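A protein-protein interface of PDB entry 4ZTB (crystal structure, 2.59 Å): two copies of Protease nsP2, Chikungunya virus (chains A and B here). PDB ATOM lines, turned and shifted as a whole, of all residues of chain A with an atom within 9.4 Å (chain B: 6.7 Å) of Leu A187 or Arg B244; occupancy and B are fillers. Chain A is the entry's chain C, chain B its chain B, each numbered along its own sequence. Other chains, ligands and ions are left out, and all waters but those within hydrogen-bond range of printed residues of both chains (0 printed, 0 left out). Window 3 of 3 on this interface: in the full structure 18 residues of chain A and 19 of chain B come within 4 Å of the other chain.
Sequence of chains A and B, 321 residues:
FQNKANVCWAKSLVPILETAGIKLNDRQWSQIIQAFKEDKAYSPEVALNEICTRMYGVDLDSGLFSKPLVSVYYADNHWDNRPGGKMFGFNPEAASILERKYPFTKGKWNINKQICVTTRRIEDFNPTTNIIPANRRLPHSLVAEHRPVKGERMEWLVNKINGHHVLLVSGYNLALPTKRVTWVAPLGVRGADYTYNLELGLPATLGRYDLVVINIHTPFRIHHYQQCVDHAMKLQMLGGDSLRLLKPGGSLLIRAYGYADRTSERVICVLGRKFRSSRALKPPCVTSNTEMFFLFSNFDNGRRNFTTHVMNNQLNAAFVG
The backbone carbonyl oxygen of Tyr A194 lies within hydrogen-bond range of the backbone NH of Ala A185, 3.0 Å away.
Leu A187 touches one residue of chain B. Of chain A, only Leu A187 and Thr A195 come within 4 Å of Arg B244. No residue of chain A comes within 4 Å of Leu B245. Of the printed residues of chain B, Gly A188 touches Tyr B74. Of the printed residues of chain B, Thr A195 touches Arg B244 (2.9 Å). Of the printed residues of chain B, Arg A190 touches Asp B241. Printed residues of chain A within 4 Å of Asn B301: Tyr A194. Printed residues of chain A within 4 Å of Asp B241: Arg A190. The nearest residue of chain B that does not touch Leu A187 is Tyr B74 (6.0 Å).
No position is printed for both chains. Of the 5 pairs that touch across the chains among the printed residues, none has its exchanged pair printed and touching as well.
OD2 of Asp B241 is in salt-bridge range of NH1 of Arg A190 (3.2 Å). NH2 of Arg B244 is in hydrogen-bond range of O of Thr A195 (2.9 Å). O of Asn B301 sits at hydrogen-bond distance from OH of Tyr A194, 2.7 Å away.
CD2 of Leu A187 touches NH2 of Arg B244, 3.4 Å away. Tyr B74 touches Gly A188 (CE2 to O, 3.4 Å).
Of the 19 printed residues of chain A, 5 touch a printed residue of chain B. Among the printed residues, 5 pairs touch across the chains. Among the printed residues, Asp or Glu carboxylates within 4 Å of a Lys or Arg side-chain nitrogen of the other chain: Arg A190 with Asp B241 (3.2 Å).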
ATOM      1  N   SER A 170       8.491 -14.684  15.511  1.00  0.00           N
ATOM      2  CA  SER A 170       9.263 -13.653  14.812  1.00  0.00           C
ATOM      3  C   SER A 170      10.636 -14.117  14.304  1.00  0.00           C
ATOM      4  O   SER A 170      11.231 -15.062  14.825  1.00  0.00           O
ATOM      5  CB  SER A 170       9.470 -12.476  15.771  1.00  0.00           C
ATOM      6  OG  SER A 170      10.088 -11.376  15.144  1.00  0.00           O
ATOM      7  N   GLY A 171      11.126 -13.434  13.282  1.00  0.00           N
ATOM      8  CA  GLY A 171      12.467 -13.652  12.755  1.00  0.00           C
ATOM      9  C   GLY A 171      13.541 -13.064  13.671  1.00  0.00           C
ATOM     10  O   GLY A 171      14.697 -13.489  13.610  1.00  0.00           O
ATOM     11  N   VAL A 184       9.587 -18.013  19.454  1.00  0.00           N
ATOM     12  CA  VAL A 184       9.534 -18.988  18.363  1.00  0.00           C
ATOM     13  C   VAL A 184      10.036 -18.269  17.097  1.00  0.00           C
ATOM     14  O   VAL A 184       9.680 -17.091  16.874  1.00  0.00           O
ATOM     15  CB  VAL A 184       8.106 -19.542  18.156  1.00  0.00           C
ATOM     16  CG1 VAL A 184       8.010 -20.448  16.922  1.00  0.00           C
ATOM     17  CG2 VAL A 184       7.651 -20.298  19.397  1.00  0.00           C
ATOM     18  N   ALA A 185      10.839 -18.961  16.274  1.00  0.00           N
ATOM     19  CA  ALA A 185      11.470 -18.349  15.071  1.00  0.00           C
ATOM     20  C   ALA A 185      11.603 -19.316  13.891  1.00  0.00           C
ATOM     21  O   ALA A 185      11.529 -20.522  14.086  1.00  0.00           O
ATOM     22  CB  ALA A 185      12.843 -17.798  15.453  1.00  0.00           C
ATOM     23  N   PRO A 186      11.801 -18.786  12.651  1.00  0.00           N
ATOM     24  CA  PRO A 186      11.990 -19.684  11.508  1.00  0.00           C
ATOM     25  C   PRO A 186      13.308 -20.436  11.630  1.00  0.00           C
ATOM     26  O   PRO A 186      14.212 -19.999  12.361  1.00  0.00           O
ATOM     27  CB  PRO A 186      11.991 -18.729  10.297  1.00  0.00           C
ATOM     28  CG  PRO A 186      12.430 -17.428  10.837  1.00  0.00           C
ATOM     29  CD  PRO A 186      11.824 -17.367  12.215  1.00  0.00           C
ATOM     30  N   LEU A 187      13.415 -21.551  10.911  1.00  0.00           N
ATOM     31  CA  LEU A 187      14.592 -22.432  10.999  1.00  0.00           C
ATOM     32  C   LEU A 187      15.889 -21.691  10.671  1.00  0.00           C
ATOM     33  O   LEU A 187      15.889 -20.760   9.875  1.00  0.00           O
ATOM     34  CB  LEU A 187      14.423 -23.664  10.098  1.00  0.00           C
ATOM     35  CG  LEU A 187      13.242 -24.596  10.423  1.00  0.00           C
ATOM     36  CD1 LEU A 187      13.125 -25.647   9.342  1.00  0.00           C
ATOM     37  CD2 LEU A 187      13.379 -25.245  11.795  1.00  0.00           C
ATOM     38  N   GLY A 188      16.984 -22.116  11.305  1.00  0.00           N
ATOM     39  CA  GLY A 188      18.294 -21.480  11.138  1.00  0.00           C
ATOM     40  C   GLY A 188      18.549 -20.238  11.984  1.00  0.00           C
ATOM     41  O   GLY A 188      19.671 -19.729  11.969  1.00  0.00           O
ATOM     42  N   VAL A 189      17.532 -19.743  12.709  1.00  0.00           N
ATOM     43  CA  VAL A 189      17.677 -18.587  13.603  1.00  0.00           C
ATOM     44  C   VAL A 189      18.183 -19.119  14.949  1.00  0.00           C
ATOM     45  O   VAL A 189      17.643 -20.099  15.479  1.00  0.00           O
ATOM     46  CB  VAL A 189      16.354 -17.790  13.769  1.00  0.00           C
ATOM     47  CG1 VAL A 189      16.502 -16.641  14.749  1.00  0.00           C
ATOM     48  CG2 VAL A 189      15.890 -17.241  12.423  1.00  0.00           C
ATOM     49  N   ARG A 190      19.220 -18.460  15.478  1.00  0.00           N
ATOM     50  CA  ARG A 190      19.845 -18.781  16.758  1.00  0.00           C
ATOM     51  C   ARG A 190      19.373 -17.752  17.770  1.00  0.00           C
ATOM     52  O   ARG A 190      18.954 -16.638  17.396  1.00  0.00           O
ATOM     53  CB  ARG A 190      21.385 -18.740  16.675  1.00  0.00           C
ATOM     54  CG  ARG A 190      22.031 -19.463  15.489  1.00  0.00           C
ATOM     55  CD  ARG A 190      21.855 -20.964  15.517  1.00  0.00           C
ATOM     56  NE  ARG A 190      22.150 -21.537  14.192  1.00  0.00           N
ATOM     57  CZ  ARG A 190      23.360 -21.851  13.709  1.00  0.00           C
ATOM     58  NH1 ARG A 190      24.468 -21.666  14.420  1.00  0.00           N
ATOM     59  NH2 ARG A 190      23.466 -22.366  12.478  1.00  0.00           N
ATOM     60  N   ALA A 192      16.789 -18.291  19.818  1.00  0.00           N
ATOM     61  CA  ALA A 192      15.359 -18.512  20.078  1.00  0.00           C
ATOM     62  C   ALA A 192      15.132 -19.703  20.971  1.00  0.00           C
ATOM     63  O   ALA A 192      15.984 -20.605  21.076  1.00  0.00           O
ATOM     64  CB  ALA A 192      14.611 -18.684  18.778  1.00  0.00           C
ATOM     65  N   ASP A 193      13.972 -19.695  21.621  1.00  0.00           N
ATOM     66  CA  ASP A 193      13.548 -20.787  22.494  1.00  0.00           C
ATOM     67  C   ASP A 193      13.170 -21.990  21.639  1.00  0.00           C
ATOM     68  O   ASP A 193      13.505 -23.121  21.987  1.00  0.00           O
ATOM     69  CB  ASP A 193      12.386 -20.359  23.384  1.00  0.00           C
ATOM     70  CG  ASP A 193      12.784 -19.278  24.355  1.00  0.00           C
ATOM     71  OD1 ASP A 193      13.700 -19.514  25.165  1.00  0.00           O
ATOM     72  OD2 ASP A 193      12.189 -18.191  24.316  1.00  0.00           O
ATOM     73  N   TYR A 194      12.476 -21.755  20.523  1.00  0.00           N
ATOM     74  CA  TYR A 194      12.115 -22.826  19.575  1.00  0.00           C
ATOM     75  C   TYR A 194      12.251 -22.337  18.144  1.00  0.00           C
ATOM     76  O   TYR A 194      12.154 -21.124  17.880  1.00  0.00           O
ATOM     77  CB  TYR A 194      10.687 -23.315  19.817  1.00  0.00           C
ATOM     78  CG  TYR A 194      10.456 -23.843  21.207  1.00  0.00           C
ATOM     79  CD1 TYR A 194      10.926 -25.106  21.575  1.00  0.00           C
ATOM     80  CD2 TYR A 194       9.765 -23.082  22.178  1.00  0.00           C
ATOM     81  CE1 TYR A 194      10.721 -25.609  22.857  1.00  0.00           C
ATOM     82  CE2 TYR A 194       9.555 -23.585  23.475  1.00  0.00           C
ATOM     83  CZ  TYR A 194      10.036 -24.847  23.802  1.00  0.00           C
ATOM     84  OH  TYR A 194       9.843 -25.350  25.055  1.00  0.00           O
ATOM     85  N   THR A 195      12.486 -23.288  17.233  1.00  0.00           N
ATOM     86  CA  THR A 195      12.544 -23.027  15.786  1.00  0.00           C
ATOM     87  C   THR A 195      11.629 -24.026  15.091  1.00  0.00           C
ATOM     88  O   THR A 195      11.642 -25.226  15.414  1.00  0.00           O
ATOM     89  CB  THR A 195      13.975 -23.094  15.208  1.00  0.00           C
ATOM     90  OG1 THR A 195      14.597 -24.313  15.608  1.00  0.00           O
ATOM     91  CG2 THR A 195      14.807 -21.934  15.711  1.00  0.00           C
ATOM     92  N   TYR A 196      10.829 -23.515  14.148  1.00  0.00           N
ATOM     93  CA  TYR A 196       9.878 -24.311  13.344  1.00  0.00           C
ATOM     94  C   TYR A 196       9.758 -23.766  11.947  1.00  0.00           C
ATOM     95  O   TYR A 196       9.962 -22.570  11.728  1.00  0.00           O
ATOM     96  CB  TYR A 196       8.476 -24.293  13.971  1.00  0.00           C
ATOM     97  CG  TYR A 196       8.377 -25.050  15.264  1.00  0.00           C
ATOM     98  CD1 TYR A 196       8.405 -26.452  15.267  1.00  0.00           C
ATOM     99  CD2 TYR A 196       8.256 -24.374  16.506  1.00  0.00           C
ATOM    100  CE1 TYR A 196       8.317 -27.171  16.453  1.00  0.00           C
ATOM    101  CE2 TYR A 196       8.168 -25.087  17.712  1.00  0.00           C
ATOM    102  CZ  TYR A 196       8.199 -26.486  17.686  1.00  0.00           C
ATOM    103  OH  TYR A 196       8.110 -27.206  18.860  1.00  0.00           O
ATOM    104  N   ASN A 197       9.423 -24.643  11.002  1.00  0.00           N
ATOM    105  CA  ASN A 197       9.146 -24.225   9.640  1.00  0.00           C
ATOM    106  C   ASN A 197       7.775 -23.578   9.716  1.00  0.00           C
ATOM    107  O   ASN A 197       6.751 -24.278   9.721  1.00  0.00           O
ATOM    108  CB  ASN A 197       9.173 -25.392   8.663  1.00  0.00           C
ATOM    109  CG  ASN A 197       8.862 -24.974   7.226  1.00  0.00           C
ATOM    110  OD1 ASN A 197       8.617 -23.798   6.925  1.00  0.00           O
ATOM    111  ND2 ASN A 197       8.871 -25.948   6.330  1.00  0.00           N
ATOM    112  N   LEU A 198       7.761 -22.244   9.777  1.00  0.00           N
ATOM    113  CA  LEU A 198       6.501 -21.482   9.949  1.00  0.00           C
ATOM    114  C   LEU A 198       5.527 -21.564   8.754  1.00  0.00           C
ATOM    115  O   LEU A 198       4.341 -21.223   8.916  1.00  0.00           O
ATOM    116  CB  LEU A 198       6.801 -20.021  10.331  1.00  0.00           C
ATOM    117  CG  LEU A 198       7.591 -19.793  11.631  1.00  0.00           C
ATOM    118  CD1 LEU A 198       7.787 -18.299  11.845  1.00  0.00           C
ATOM    119  CD2 LEU A 198       6.930 -20.413  12.856  1.00  0.00           C
ATOM    120  N   GLU A 199       6.001 -22.020   7.571  1.00  0.00           N
ATOM    121  CA  GLU A 199       5.087 -22.299   6.420  1.00  0.00           C
ATOM    122  C   GLU A 199       4.248 -23.589   6.655  1.00  0.00           C
ATOM    123  O   GLU A 199       3.455 -23.932   5.800  1.00  0.00           O
ATOM    124  CB  GLU A 199       5.808 -22.363   5.038  1.00  0.00           C
ATOM    125  CG  GLU A 199       6.103 -20.967   4.421  1.00  0.00           C
ATOM    126  CD  GLU A 199       7.256 -20.204   5.080  1.00  0.00           C
ATOM    127  OE1 GLU A 199       8.191 -20.840   5.641  1.00  0.00           O
ATOM    128  OE2 GLU A 199       7.236 -18.947   5.029  1.00  0.00           O
ATOM    129  N   LEU A 200       4.452 -24.301   7.788  1.00  0.00           N
ATOM    130  CA  LEU A 200       3.627 -25.435   8.221  1.00  0.00           C
ATOM    131  C   LEU A 200       2.778 -25.089   9.477  1.00  0.00           C
ATOM    132  O   LEU A 200       2.175 -25.983  10.074  1.00  0.00           O
ATOM    133  CB  LEU A 200       4.512 -26.650   8.506  1.00  0.00           C
ATOM    134  CG  LEU A 200       5.414 -27.140   7.369  1.00  0.00           C
ATOM    135  CD1 LEU A 200       6.319 -28.249   7.887  1.00  0.00           C
ATOM    136  CD2 LEU A 200       4.620 -27.617   6.154  1.00  0.00           C
ATOM    137  N   ILE A 216       5.641 -11.653  11.731  1.00  0.00           N
ATOM    138  CA  ILE A 216       6.297 -12.063  10.489  1.00  0.00           C
ATOM    139  C   ILE A 216       5.963 -11.007   9.437  1.00  0.00           C
ATOM    140  O   ILE A 216       4.811 -10.591   9.308  1.00  0.00           O
ATOM    141  CB  ILE A 216       5.892 -13.480  10.032  1.00  0.00           C
ATOM    142  CG1 ILE A 216       6.229 -14.525  11.108  1.00  0.00           C
ATOM    143  CG2 ILE A 216       6.593 -13.858   8.731  1.00  0.00           C
ATOM    144  CD1 ILE A 216       7.708 -14.670  11.467  1.00  0.00           C
ATOM    145  N   TYR B  74      19.030 -12.207   7.989  1.00  0.00           N
ATOM    146  CA  TYR B  74      19.805 -13.444   7.827  1.00  0.00           C
ATOM    147  C   TYR B  74      19.087 -14.417   6.908  1.00  0.00           C
ATOM    148  O   TYR B  74      17.928 -14.742   7.158  1.00  0.00           O
ATOM    149  CB  TYR B  74      20.035 -14.078   9.190  1.00  0.00           C
ATOM    150  CG  TYR B  74      20.861 -15.336   9.153  1.00  0.00           C
ATOM    151  CD1 TYR B  74      22.191 -15.307   8.703  1.00  0.00           C
ATOM    152  CD2 TYR B  74      20.324 -16.571   9.572  1.00  0.00           C
ATOM    153  CE1 TYR B  74      22.966 -16.471   8.665  1.00  0.00           C
ATOM    154  CE2 TYR B  74      21.088 -17.740   9.542  1.00  0.00           C
ATOM    155  CZ  TYR B  74      22.405 -17.688   9.091  1.00  0.00           C
ATOM    156  OH  TYR B  74      23.149 -18.835   9.063  1.00  0.00           O
ATOM    157  N   PRO B 203      25.393 -29.558  12.715  1.00  0.00           N
ATOM    158  CA  PRO B 203      24.214 -29.964  11.949  1.00  0.00           C
ATOM    159  C   PRO B 203      23.356 -31.005  12.693  1.00  0.00           C
ATOM    160  O   PRO B 203      23.902 -31.946  13.300  1.00  0.00           O
ATOM    161  CB  PRO B 203      24.818 -30.568  10.675  1.00  0.00           C
ATOM    162  CG  PRO B 203      26.102 -31.144  11.117  1.00  0.00           C
ATOM    163  CD  PRO B 203      26.611 -30.227  12.213  1.00  0.00           C
ATOM    164  N   ALA B 204      22.028 -30.823  12.628  1.00  0.00           N
ATOM    165  CA  ALA B 204      21.034 -31.741  13.243  1.00  0.00           C
ATOM    166  C   ALA B 204      21.186 -33.218  12.799  1.00  0.00           C
ATOM    167  O   ALA B 204      20.832 -34.129  13.560  1.00  0.00           O
ATOM    168  CB  ALA B 204      19.613 -31.251  12.952  1.00  0.00           C
ATOM    169  N   GLY B 207      22.364 -36.429  14.997  1.00  0.00           N
ATOM    170  CA  GLY B 207      21.484 -37.246  15.842  1.00  0.00           C
ATOM    171  C   GLY B 207      21.481 -36.810  17.285  1.00  0.00           C
ATOM    172  O   GLY B 207      22.201 -35.876  17.660  1.00  0.00           O
ATOM    173  N   ARG B 208      20.669 -37.492  18.090  1.00  0.00           N
ATOM    174  CA  ARG B 208      20.486 -37.169  19.515  1.00  0.00           C
ATOM    175  C   ARG B 208      21.307 -38.092  20.407  1.00  0.00           C
ATOM    176  O   ARG B 208      21.452 -39.287  20.129  1.00  0.00           O
ATOM    177  CB  ARG B 208      19.000 -37.198  19.875  1.00  0.00           C
ATOM    178  CG  ARG B 208      18.217 -36.091  19.179  1.00  0.00           C
ATOM    179  CD  ARG B 208      16.713 -36.114  19.457  1.00  0.00           C
ATOM    180  NE  ARG B 208      16.024 -34.972  18.769  1.00  0.00           N
ATOM    181  CZ  ARG B 208      15.988 -33.686  19.200  1.00  0.00           C
ATOM    182  NH1 ARG B 208      16.605 -33.291  20.340  1.00  0.00           N
ATOM    183  NH2 ARG B 208      15.325 -32.761  18.476  1.00  0.00           N
ATOM    184  N   TYR B 209      21.837 -37.505  21.487  1.00  0.00           N
ATOM    185  CA  TYR B 209      22.748 -38.163  22.417  1.00  0.00           C
ATOM    186  C   TYR B 209      22.357 -37.962  23.876  1.00  0.00           C
ATOM    187  O   TYR B 209      21.577 -37.065  24.201  1.00  0.00           O
ATOM    188  CB  TYR B 209      24.145 -37.591  22.196  1.00  0.00           C
ATOM    189  CG  TYR B 209      24.693 -37.818  20.795  1.00  0.00           C
ATOM    190  CD1 TYR B 209      24.452 -36.904  19.763  1.00  0.00           C
ATOM    191  CD2 TYR B 209      25.457 -38.955  20.506  1.00  0.00           C
ATOM    192  CE1 TYR B 209      24.963 -37.125  18.481  1.00  0.00           C
ATOM    193  CE2 TYR B 209      25.967 -39.183  19.236  1.00  0.00           C
ATOM    194  CZ  TYR B 209      25.719 -38.274  18.227  1.00  0.00           C
ATOM    195  OH  TYR B 209      26.229 -38.512  16.973  1.00  0.00           O
ATOM    196  N   GLY B 239      26.376 -24.213  21.596  1.00  0.00           N
ATOM    197  CA  GLY B 239      25.436 -24.475  22.707  1.00  0.00           C
ATOM    198  C   GLY B 239      23.984 -24.538  22.252  1.00  0.00           C
ATOM    199  O   GLY B 239      23.243 -25.419  22.657  1.00  0.00           O
ATOM    200  N   GLY B 240      23.588 -23.594  21.405  1.00  0.00           N
ATOM    201  CA  GLY B 240      22.228 -23.529  20.849  1.00  0.00           C
ATOM    202  C   GLY B 240      21.925 -24.690  19.937  1.00  0.00           C
ATOM    203  O   GLY B 240      20.882 -25.330  20.076  1.00  0.00           O
ATOM    204  N   ASP B 241      22.835 -24.968  19.001  1.00  0.00           N
ATOM    205  CA  ASP B 241      22.675 -26.100  18.046  1.00  0.00           C
ATOM    206  C   ASP B 241      22.710 -27.476  18.706  1.00  0.00           C
ATOM    207  O   ASP B 241      22.196 -28.444  18.120  1.00  0.00           O
ATOM    208  CB  ASP B 241      23.727 -26.043  16.926  1.00  0.00           C
ATOM    209  CG  ASP B 241      23.529 -24.853  15.985  1.00  0.00           C
ATOM    210  OD1 ASP B 241      22.655 -24.000  16.205  1.00  0.00           O
ATOM    211  OD2 ASP B 241      24.263 -24.780  15.007  1.00  0.00           O
ATOM    212  N   SER B 242      23.310 -27.570  19.900  1.00  0.00           N
ATOM    213  CA  SER B 242      23.288 -28.813  20.692  1.00  0.00           C
ATOM    214  C   SER B 242      21.886 -29.204  21.177  1.00  0.00           C
ATOM    215  O   SER B 242      21.654 -30.378  21.436  1.00  0.00           O
ATOM    216  CB  SER B 242      24.218 -28.710  21.898  1.00  0.00           C
ATOM    217  OG  SER B 242      25.547 -28.532  21.463  1.00  0.00           O
ATOM    218  N   LEU B 243      20.965 -28.236  21.297  1.00  0.00           N
ATOM    219  CA  LEU B 243      19.561 -28.496  21.742  1.00  0.00           C
ATOM    220  C   LEU B 243      18.799 -29.531  20.865  1.00  0.00           C
ATOM    221  O   LEU B 243      17.969 -30.287  21.393  1.00  0.00           O
ATOM    222  CB  LEU B 243      18.767 -27.175  21.854  1.00  0.00           C
ATOM    223  CG  LEU B 243      19.287 -26.086  22.830  1.00  0.00           C
ATOM    224  CD1 LEU B 243      18.413 -24.842  22.771  1.00  0.00           C
ATOM    225  CD2 LEU B 243      19.372 -26.598  24.260  1.00  0.00           C
ATOM    226  N   ARG B 244      19.090 -29.562  19.549  1.00  0.00           N
ATOM    227  CA  ARG B 244      18.520 -30.580  18.603  1.00  0.00           C
ATOM    228  C   ARG B 244      19.341 -31.911  18.542  1.00  0.00           C
ATOM    229  O   ARG B 244      19.021 -32.808  17.753  1.00  0.00           O
ATOM    230  CB  ARG B 244      18.348 -29.976  17.193  1.00  0.00           C
ATOM    231  CG  ARG B 244      17.189 -28.986  17.085  1.00  0.00           C
ATOM    232  CD  ARG B 244      17.162 -28.266  15.733  1.00  0.00           C
ATOM    233  NE  ARG B 244      15.952 -27.438  15.495  1.00  0.00           N
ATOM    234  CZ  ARG B 244      14.831 -27.816  14.836  1.00  0.00           C
ATOM    235  NH1 ARG B 244      14.684 -29.051  14.304  1.00  0.00           N
ATOM    236  NH2 ARG B 244      13.817 -26.934  14.706  1.00  0.00           N
ATOM    237  N   LEU B 245      20.384 -32.017  19.379  1.00  0.00           N
ATOM    238  CA  LEU B 245      21.263 -33.173  19.480  1.00  0.00           C
ATOM    239  C   LEU B 245      21.203 -33.810  20.883  1.00  0.00           C
ATOM    240  O   LEU B 245      22.192 -34.420  21.327  1.00  0.00           O
ATOM    241  CB  LEU B 245      22.707 -32.744  19.173  1.00  0.00           C
ATOM    242  CG  LEU B 245      22.968 -31.925  17.910  1.00  0.00           C
ATOM    243  CD1 LEU B 245      24.432 -31.535  17.860  1.00  0.00           C
ATOM    244  CD2 LEU B 245      22.570 -32.698  16.666  1.00  0.00           C
ATOM    245  N   LEU B 246      20.053 -33.679  21.564  1.00  0.00           N
ATOM    246  CA  LEU B 246      19.848 -34.222  22.913  1.00  0.00           C
ATOM    247  C   LEU B 246      18.600 -35.091  23.014  1.00  0.00           C
ATOM    248  O   LEU B 246      17.489 -34.643  22.669  1.00  0.00           O
ATOM    249  CB  LEU B 246      19.735 -33.080  23.918  1.00  0.00           C
ATOM    250  CG  LEU B 246      21.032 -32.353  24.250  1.00  0.00           C
ATOM    251  CD1 LEU B 246      20.751 -31.018  24.907  1.00  0.00           C
ATOM    252  CD2 LEU B 246      21.921 -33.200  25.155  1.00  0.00           C
ATOM    253  N   LYS B 247      18.785 -36.335  23.484  1.00  0.00           N
ATOM    254  CA  LYS B 247      17.664 -37.235  23.735  1.00  0.00           C
ATOM    255  C   LYS B 247      16.970 -36.773  25.003  1.00  0.00           C
ATOM    256  O   LYS B 247      17.592 -36.044  25.804  1.00  0.00           O
ATOM    257  CB  LYS B 247      18.106 -38.688  23.884  1.00  0.00           C
ATOM    258  CG  LYS B 247      18.631 -39.305  22.600  1.00  0.00           C
ATOM    259  CD  LYS B 247      18.649 -40.830  22.617  1.00  0.00           C
ATOM    260  CE  LYS B 247      19.518 -41.383  23.724  1.00  0.00           C
ATOM    261  NZ  LYS B 247      19.725 -42.849  23.582  1.00  0.00           N
ATOM    262  N   PHE B 299      17.517 -32.832  30.098  1.00  0.00           N
ATOM    263  CA  PHE B 299      16.859 -32.086  29.025  1.00  0.00           C
ATOM    264  C   PHE B 299      15.422 -32.529  28.791  1.00  0.00           C
ATOM    265  O   PHE B 299      15.187 -33.720  28.611  1.00  0.00           O
ATOM    266  CB  PHE B 299      17.665 -32.300  27.728  1.00  0.00           C
ATOM    267  CG  PHE B 299      17.112 -31.601  26.505  1.00  0.00           C
ATOM    268  CD1 PHE B 299      17.225 -30.213  26.360  1.00  0.00           C
ATOM    269  CD2 PHE B 299      16.492 -32.331  25.483  1.00  0.00           C
ATOM    270  CE1 PHE B 299      16.720 -29.567  25.226  1.00  0.00           C
ATOM    271  CE2 PHE B 299      15.985 -31.694  24.345  1.00  0.00           C
ATOM    272  CZ  PHE B 299      16.100 -30.311  24.218  1.00  0.00           C
ATOM    273  N   ASN B 301      13.379 -30.113  26.680  1.00  0.00           N
ATOM    274  CA  ASN B 301      13.013 -29.142  25.628  1.00  0.00           C
ATOM    275  C   ASN B 301      11.865 -28.203  26.069  1.00  0.00           C
ATOM    276  O   ASN B 301      11.064 -27.734  25.238  1.00  0.00           O
ATOM    277  CB  ASN B 301      12.682 -29.878  24.315  1.00  0.00           C
ATOM    278  CG  ASN B 301      12.668 -28.963  23.078  1.00  0.00           C
ATOM    279  OD1 ASN B 301      11.762 -29.090  22.269  1.00  0.00           O
ATOM    280  ND2 ASN B 301      13.654 -28.048  22.925  1.00  0.00           N
